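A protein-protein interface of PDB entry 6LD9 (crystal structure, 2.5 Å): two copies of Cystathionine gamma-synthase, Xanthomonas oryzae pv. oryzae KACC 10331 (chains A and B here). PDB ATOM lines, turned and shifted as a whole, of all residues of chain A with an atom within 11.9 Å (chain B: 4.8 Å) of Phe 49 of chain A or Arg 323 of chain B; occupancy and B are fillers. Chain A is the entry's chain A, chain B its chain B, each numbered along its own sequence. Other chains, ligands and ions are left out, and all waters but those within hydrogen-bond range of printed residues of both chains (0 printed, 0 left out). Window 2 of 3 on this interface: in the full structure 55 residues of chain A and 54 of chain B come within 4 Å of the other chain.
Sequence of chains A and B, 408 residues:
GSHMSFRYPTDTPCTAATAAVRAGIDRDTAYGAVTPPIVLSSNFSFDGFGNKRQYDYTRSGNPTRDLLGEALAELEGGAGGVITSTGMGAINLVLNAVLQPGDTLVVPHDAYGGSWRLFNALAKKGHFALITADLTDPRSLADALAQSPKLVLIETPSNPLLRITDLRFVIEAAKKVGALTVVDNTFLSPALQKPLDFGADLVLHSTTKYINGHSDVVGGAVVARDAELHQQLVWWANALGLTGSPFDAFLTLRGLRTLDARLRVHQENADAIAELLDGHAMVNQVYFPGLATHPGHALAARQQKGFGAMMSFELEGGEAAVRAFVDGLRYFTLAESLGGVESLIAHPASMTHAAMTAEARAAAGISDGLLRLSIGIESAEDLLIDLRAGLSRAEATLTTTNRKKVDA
The guanidinium group (NE) of Arg 53 of chain A sits at hydrogen-bond distance from the backbone carbonyl oxygen (O) of Ser 45 of chain A (2.9 Å). The backbone carbonyl oxygen (O) of Phe 46 of chain A lies within hydrogen-bond range of the guanidinium group (NH2) of Arg 53 of chain A (3.5 Å). The side-chain carboxylate of Glu 319 of chain B is in salt-bridge range of the guanidinium group of Arg 323 of chain B (3.6 Å).
Among the printed residues, merely in contact across the chains: Ser 45 of chain A with Leu 334 of chain B (3.4 Å), Gly 48 of chain A with Asp 327 of chain B (3.3 Å), Gly 48 of chain A with Leu 334 of chain B (3.6 Å), Phe 49 of chain A with Val 322 of chain B (3.6 Å), Phe 49 of chain A with Arg 323 of chain B (3.8 Å), Phe 49 of chain A with Leu 334 of chain B (3.5 Å) and Phe 49 of chain A with His 347 of chain B (3.7 Å).
No position is printed for both chains. Of the 9 pairs that touch across the chains among the printed residues, none has its exchanged pair printed and touching as well.
Of the printed residues of chain B, Ser 45 of chain A touches Leu 334 (3.4 Å). Of the printed residues of chain B, Phe 46 of chain A touches Leu 334 (2.9 Å). Printed residues of chain B within 4 Å of Gly 48 of chain A: Asp 327 and Leu 334. Phe 49 of chain A touches just these residues of chain B: Val 322, Arg 323, Asp 327, Leu 334 and His 347. No residue of chain A comes within 4 Å of Glu 319 of chain B. Arg 323 of chain B touches just one residue of chain A: Phe 49 (3.8 Å). No residue of chain A comes within 4 Å of Ala 324 of chain B. No residue of chain A comes within 4 Å of Val 326 of chain B. Printed residues of chain A within 4 Å of Leu 334 of chain B: Ser 45 (3.4 Å), Phe 46 (2.9 Å), Gly 48 (3.6 Å) and Phe 49 (3.5 Å). His 347 of chain B touches one residue of chain A. The nearest residue of chain B that does not touch Phe 49 of chain A is Glu 319 of chain B (4.2 Å). The nearest residue of chain A that does not touch Arg 323 of chain B is Gly 50 of chain A (5.4 Å). The nearest printed residue of chain B that does not touch Ser 45 of chain A is Val 326 of chain B (9.8 Å).
Hydrophobic or aromatic side chains of chain A within 4 Å of the printed part of chain B: Phe 46 and Phe 49. Of the 11 printed residues of chain B, 5 touch a printed residue of chain A. Printed residues of chain B that touch a printed residue of chain A: Val 322, Arg 323, Asp 327, Leu 334 and His 347. Among the printed residues, no Asp or Glu carboxylate lies within 4 Å of a Lys or Arg side-chain nitrogen of the other chain.
O of Leu 334 of chain B is in hydrogen-bond range of N of Phe 46 of chain A (2.9 Å). OD1 of Asp 327 of chain B sits at hydrogen-bond distance from N of Phe 49 of chain A, 3.0 Å away.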
ATOM      1  N   PHE A  44     -11.306 -12.998 -17.828  1.00  0.00           N
ATOM      2  CA  PHE A  44     -11.929 -11.671 -17.572  1.00  0.00           C
ATOM      3  C   PHE A  44     -13.420 -11.816 -17.913  1.00  0.00           C
ATOM      4  O   PHE A  44     -13.729 -12.426 -18.937  1.00  0.00           O
ATOM      5  CB  PHE A  44     -11.177 -10.608 -18.388  1.00  0.00           C
ATOM      6  CG  PHE A  44      -9.699 -10.548 -18.111  1.00  0.00           C
ATOM      7  CD1 PHE A  44      -8.839 -11.438 -18.693  1.00  0.00           C
ATOM      8  CD2 PHE A  44      -9.168  -9.620 -17.232  1.00  0.00           C
ATOM      9  CE1 PHE A  44      -7.500 -11.417 -18.395  1.00  0.00           C
ATOM     10  CE2 PHE A  44      -7.806  -9.573 -16.939  1.00  0.00           C
ATOM     11  CZ  PHE A  44      -6.980 -10.493 -17.500  1.00  0.00           C
ATOM     12  N   SER A  45     -14.329 -11.315 -17.090  1.00  0.00           N
ATOM     13  CA  SER A  45     -15.780 -11.361 -17.414  1.00  0.00           C
ATOM     14  C   SER A  45     -16.067 -10.575 -18.682  1.00  0.00           C
ATOM     15  O   SER A  45     -15.339  -9.629 -18.962  1.00  0.00           O
ATOM     16  CB  SER A  45     -16.620 -10.822 -16.326  1.00  0.00           C
ATOM     17  OG  SER A  45     -16.160  -9.537 -16.000  1.00  0.00           O
ATOM     18  N   PHE A  46     -17.066 -11.018 -19.452  1.00  0.00           N
ATOM     19  CA  PHE A  46     -17.784 -10.173 -20.437  1.00  0.00           C
ATOM     20  C   PHE A  46     -18.684  -9.158 -19.712  1.00  0.00           C
ATOM     21  O   PHE A  46     -18.978  -9.322 -18.538  1.00  0.00           O
ATOM     22  CB  PHE A  46     -18.547 -11.036 -21.434  1.00  0.00           C
ATOM     23  CG  PHE A  46     -17.671 -11.589 -22.523  1.00  0.00           C
ATOM     24  CD1 PHE A  46     -16.412 -12.123 -22.206  1.00  0.00           C
ATOM     25  CD2 PHE A  46     -18.096 -11.599 -23.847  1.00  0.00           C
ATOM     26  CE1 PHE A  46     -15.594 -12.650 -23.203  1.00  0.00           C
ATOM     27  CE2 PHE A  46     -17.261 -12.101 -24.842  1.00  0.00           C
ATOM     28  CZ  PHE A  46     -16.029 -12.647 -24.520  1.00  0.00           C
ATOM     29  N   ASP A  47     -18.988  -8.050 -20.385  1.00  0.00           N
ATOM     30  CA  ASP A  47     -19.864  -6.943 -19.900  1.00  0.00           C
ATOM     31  C   ASP A  47     -21.290  -7.212 -20.408  1.00  0.00           C
ATOM     32  O   ASP A  47     -21.818  -6.440 -21.187  1.00  0.00           O
ATOM     33  CB  ASP A  47     -19.237  -5.610 -20.312  1.00  0.00           C
ATOM     34  CG  ASP A  47     -19.958  -4.381 -19.797  1.00  0.00           C
ATOM     35  OD1 ASP A  47     -20.634  -4.494 -18.714  1.00  0.00           O
ATOM     36  OD2 ASP A  47     -19.844  -3.326 -20.509  1.00  0.00           O
ATOM     37  N   GLY A  48     -21.833  -8.362 -20.026  1.00  0.00           N
ATOM     38  CA  GLY A  48     -23.049  -8.945 -20.603  1.00  0.00           C
ATOM     39  C   GLY A  48     -22.808  -9.614 -21.943  1.00  0.00           C
ATOM     40  O   GLY A  48     -21.761  -9.379 -22.603  1.00  0.00           O
ATOM     41  N   PHE A  49     -23.797 -10.400 -22.358  1.00  0.00           N
ATOM     42  CA  PHE A  49     -23.784 -11.174 -23.617  1.00  0.00           C
ATOM     43  C   PHE A  49     -23.261 -10.306 -24.784  1.00  0.00           C
ATOM     44  O   PHE A  49     -23.797  -9.206 -25.027  1.00  0.00           O
ATOM     45  CB  PHE A  49     -25.180 -11.759 -23.867  1.00  0.00           C
ATOM     46  CG  PHE A  49     -25.145 -12.803 -24.952  1.00  0.00           C
ATOM     47  CD1 PHE A  49     -24.530 -14.024 -24.726  1.00  0.00           C
ATOM     48  CD2 PHE A  49     -25.636 -12.535 -26.224  1.00  0.00           C
ATOM     49  CE1 PHE A  49     -24.479 -14.967 -25.744  1.00  0.00           C
ATOM     50  CE2 PHE A  49     -25.583 -13.477 -27.234  1.00  0.00           C
ATOM     51  CZ  PHE A  49     -25.002 -14.692 -26.989  1.00  0.00           C
ATOM     52  N   GLY A  50     -22.241 -10.807 -25.493  1.00  0.00           N
ATOM     53  CA  GLY A  50     -21.698 -10.246 -26.749  1.00  0.00           C
ATOM     54  C   GLY A  50     -20.687  -9.121 -26.542  1.00  0.00           C
ATOM     55  O   GLY A  50     -20.218  -8.619 -27.538  1.00  0.00           O
ATOM     56  N   ASN A  51     -20.348  -8.743 -25.300  1.00  0.00           N
ATOM     57  CA  ASN A  51     -19.533  -7.531 -24.993  1.00  0.00           C
ATOM     58  C   ASN A  51     -18.204  -7.891 -24.347  1.00  0.00           C
ATOM     59  O   ASN A  51     -18.105  -7.793 -23.126  1.00  0.00           O
ATOM     60  CB  ASN A  51     -20.223  -6.573 -24.018  1.00  0.00           C
ATOM     61  CG  ASN A  51     -21.512  -6.019 -24.582  1.00  0.00           C
ATOM     62  OD1 ASN A  51     -22.457  -5.865 -23.827  1.00  0.00           O
ATOM     63  ND2 ASN A  51     -21.577  -5.814 -25.900  1.00  0.00           N
ATOM     64  N   LYS A  52     -17.228  -8.265 -25.156  1.00  0.00           N
ATOM     65  CA  LYS A  52     -15.835  -8.482 -24.710  1.00  0.00           C
ATOM     66  C   LYS A  52     -15.359  -7.189 -24.052  1.00  0.00           C
ATOM     67  O   LYS A  52     -15.629  -6.163 -24.568  1.00  0.00           O
ATOM     68  CB  LYS A  52     -14.989  -8.828 -25.926  1.00  0.00           C
ATOM     69  CG  LYS A  52     -13.779  -9.668 -25.620  1.00  0.00           C
ATOM     70  CD  LYS A  52     -13.081 -10.155 -26.864  1.00  0.00           C
ATOM     71  CE  LYS A  52     -12.343  -9.063 -27.611  1.00  0.00           C
ATOM     72  NZ  LYS A  52     -11.564  -8.219 -26.678  1.00  0.00           N
ATOM     73  N   ARG A  53     -14.707  -7.236 -22.909  1.00  0.00           N
ATOM     74  CA  ARG A  53     -13.960  -6.057 -22.398  1.00  0.00           C
ATOM     75  C   ARG A  53     -12.651  -5.922 -23.195  1.00  0.00           C
ATOM     76  O   ARG A  53     -12.465  -6.650 -24.153  1.00  0.00           O
ATOM     77  CB  ARG A  53     -13.684  -6.234 -20.903  1.00  0.00           C
ATOM     78  CG  ARG A  53     -14.952  -6.399 -20.094  1.00  0.00           C
ATOM     79  CD  ARG A  53     -14.585  -6.430 -18.658  1.00  0.00           C
ATOM     80  NE  ARG A  53     -15.680  -6.959 -17.861  1.00  0.00           N
ATOM     81  CZ  ARG A  53     -16.644  -6.239 -17.291  1.00  0.00           C
ATOM     82  NH1 ARG A  53     -16.728  -4.956 -17.540  1.00  0.00           N
ATOM     83  NH2 ARG A  53     -17.599  -6.822 -16.592  1.00  0.00           N
ATOM     84  N   GLU B 319     -32.059 -16.212 -30.118  1.00  0.00           N
ATOM     85  CA  GLU B 319     -30.987 -15.381 -29.546  1.00  0.00           C
ATOM     86  C   GLU B 319     -31.588 -14.548 -28.408  1.00  0.00           C
ATOM     87  O   GLU B 319     -30.886 -14.306 -27.426  1.00  0.00           O
ATOM     88  CB  GLU B 319     -30.301 -14.567 -30.645  1.00  0.00           C
ATOM     89  CG  GLU B 319     -29.043 -13.862 -30.129  1.00  0.00           C
ATOM     90  CD  GLU B 319     -28.129 -13.192 -31.150  1.00  0.00           C
ATOM     91  OE1 GLU B 319     -26.908 -13.551 -31.189  1.00  0.00           O
ATOM     92  OE2 GLU B 319     -28.617 -12.304 -31.888  1.00  0.00           O
ATOM     93  N   ALA B 320     -32.860 -14.163 -28.488  1.00  0.00           N
ATOM     94  CA  ALA B 320     -33.555 -13.414 -27.399  1.00  0.00           C
ATOM     95  C   ALA B 320     -33.475 -14.244 -26.108  1.00  0.00           C
ATOM     96  O   ALA B 320     -33.276 -13.647 -25.027  1.00  0.00           O
ATOM     97  CB  ALA B 320     -35.013 -13.091 -27.740  1.00  0.00           C
ATOM     98  N   ALA B 321     -33.689 -15.560 -26.211  1.00  0.00           N
ATOM     99  CA  ALA B 321     -33.776 -16.433 -25.028  1.00  0.00           C
ATOM    100  C   ALA B 321     -32.385 -16.568 -24.398  1.00  0.00           C
ATOM    101  O   ALA B 321     -32.291 -16.478 -23.171  1.00  0.00           O
ATOM    102  CB  ALA B 321     -34.290 -17.766 -25.438  1.00  0.00           C
ATOM    103  N   VAL B 322     -31.360 -16.797 -25.221  1.00  0.00           N
ATOM    104  CA  VAL B 322     -29.960 -16.910 -24.749  1.00  0.00           C
ATOM    105  C   VAL B 322     -29.629 -15.659 -23.924  1.00  0.00           C
ATOM    106  O   VAL B 322     -29.142 -15.817 -22.790  1.00  0.00           O
ATOM    107  CB  VAL B 322     -29.012 -17.065 -25.945  1.00  0.00           C
ATOM    108  CG1 VAL B 322     -27.575 -16.881 -25.518  1.00  0.00           C
ATOM    109  CG2 VAL B 322     -29.173 -18.402 -26.675  1.00  0.00           C
ATOM    110  N   ARG B 323     -29.924 -14.473 -24.468  1.00  0.00           N
ATOM    111  CA  ARG B 323     -29.580 -13.157 -23.882  1.00  0.00           C
ATOM    112  C   ARG B 323     -30.336 -13.032 -22.559  1.00  0.00           C
ATOM    113  O   ARG B 323     -29.709 -12.672 -21.549  1.00  0.00           O
ATOM    114  CB  ARG B 323     -29.855 -11.989 -24.852  1.00  0.00           C
ATOM    115  CG  ARG B 323     -29.371 -10.608 -24.373  1.00  0.00           C
ATOM    116  CD  ARG B 323     -29.270  -9.473 -25.404  1.00  0.00           C
ATOM    117  NE  ARG B 323     -29.192 -10.010 -26.784  1.00  0.00           N
ATOM    118  CZ  ARG B 323     -28.162  -9.875 -27.650  1.00  0.00           C
ATOM    119  NH1 ARG B 323     -27.069  -9.205 -27.329  1.00  0.00           N
ATOM    120  NH2 ARG B 323     -28.215 -10.441 -28.848  1.00  0.00           N
ATOM    121  N   ALA B 324     -31.632 -13.323 -22.518  1.00  0.00           N
ATOM    122  CA  ALA B 324     -32.393 -13.166 -21.259  1.00  0.00           C
ATOM    123  C   ALA B 324     -31.810 -14.158 -20.223  1.00  0.00           C
ATOM    124  O   ALA B 324     -31.613 -13.780 -19.063  1.00  0.00           O
ATOM    125  CB  ALA B 324     -33.889 -13.338 -21.500  1.00  0.00           C
ATOM    126  N   PHE B 325     -31.477 -15.380 -20.643  1.00  0.00           N
ATOM    127  CA  PHE B 325     -30.873 -16.416 -19.766  1.00  0.00           C
ATOM    128  C   PHE B 325     -29.545 -15.874 -19.179  1.00  0.00           C
ATOM    129  O   PHE B 325     -29.395 -15.878 -17.947  1.00  0.00           O
ATOM    130  CB  PHE B 325     -30.739 -17.741 -20.519  1.00  0.00           C
ATOM    131  CG  PHE B 325     -30.108 -18.825 -19.703  1.00  0.00           C
ATOM    132  CD1 PHE B 325     -28.730 -18.866 -19.538  1.00  0.00           C
ATOM    133  CD2 PHE B 325     -30.905 -19.723 -19.021  1.00  0.00           C
ATOM    134  CE1 PHE B 325     -28.159 -19.828 -18.729  1.00  0.00           C
ATOM    135  CE2 PHE B 325     -30.337 -20.702 -18.236  1.00  0.00           C
ATOM    136  CZ  PHE B 325     -28.970 -20.743 -18.075  1.00  0.00           C
ATOM    137  N   VAL B 326     -28.660 -15.316 -19.999  1.00  0.00           N
ATOM    138  CA  VAL B 326     -27.274 -14.976 -19.571  1.00  0.00           C
ATOM    139  C   VAL B 326     -27.243 -13.711 -18.716  1.00  0.00           C
ATOM    140  O   VAL B 326     -26.551 -13.746 -17.685  1.00  0.00           O
ATOM    141  CB  VAL B 326     -26.339 -14.858 -20.775  1.00  0.00           C
ATOM    142  CG1 VAL B 326     -24.990 -14.257 -20.399  1.00  0.00           C
ATOM    143  CG2 VAL B 326     -26.153 -16.225 -21.420  1.00  0.00           C
ATOM    144  N   ASP B 327     -27.986 -12.673 -19.086  1.00  0.00           N
ATOM    145  CA  ASP B 327     -27.983 -11.357 -18.384  1.00  0.00           C
ATOM    146  C   ASP B 327     -28.888 -11.541 -17.160  1.00  0.00           C
ATOM    147  O   ASP B 327     -30.006 -11.917 -17.345  1.00  0.00           O
ATOM    148  CB  ASP B 327     -28.272 -10.183 -19.342  1.00  0.00           C
ATOM    149  CG  ASP B 327     -27.248  -9.992 -20.509  1.00  0.00           C
ATOM    150  OD1 ASP B 327     -26.034 -10.403 -20.362  1.00  0.00           O
ATOM    151  OD2 ASP B 327     -27.652  -9.450 -21.614  1.00  0.00           O
ATOM    152  N   LEU B 334     -20.007 -14.877 -16.979  1.00  0.00           N
ATOM    153  CA  LEU B 334     -19.859 -15.002 -18.436  1.00  0.00           C
ATOM    154  C   LEU B 334     -18.401 -14.741 -18.781  1.00  0.00           C
ATOM    155  O   LEU B 334     -17.966 -13.603 -18.611  1.00  0.00           O
ATOM    156  CB  LEU B 334     -20.798 -14.001 -19.070  1.00  0.00           C
ATOM    157  CG  LEU B 334     -20.689 -13.993 -20.590  1.00  0.00           C
ATOM    158  CD1 LEU B 334     -20.974 -15.357 -21.196  1.00  0.00           C
ATOM    159  CD2 LEU B 334     -21.583 -12.908 -21.175  1.00  0.00           C
ATOM    160  N   HIS B 347     -20.363 -18.942 -24.506  1.00  0.00           N
ATOM    161  CA  HIS B 347     -21.107 -19.009 -25.797  1.00  0.00           C
ATOM    162  C   HIS B 347     -20.062 -19.306 -26.860  1.00  0.00           C
ATOM    163  O   HIS B 347     -19.338 -18.387 -27.281  1.00  0.00           O
ATOM    164  CB  HIS B 347     -21.855 -17.706 -26.041  1.00  0.00           C
ATOM    165  CG  HIS B 347     -22.601 -17.713 -27.325  1.00  0.00           C
ATOM    166  ND1 HIS B 347     -22.195 -16.956 -28.417  1.00  0.00           N
ATOM    167  CD2 HIS B 347     -23.750 -18.328 -27.672  1.00  0.00           C
ATOM    168  CE1 HIS B 347     -23.025 -17.162 -29.403  1.00  0.00           C
ATOM    169  NE2 HIS B 347     -23.990 -18.006 -28.978  1.00  0.00           N
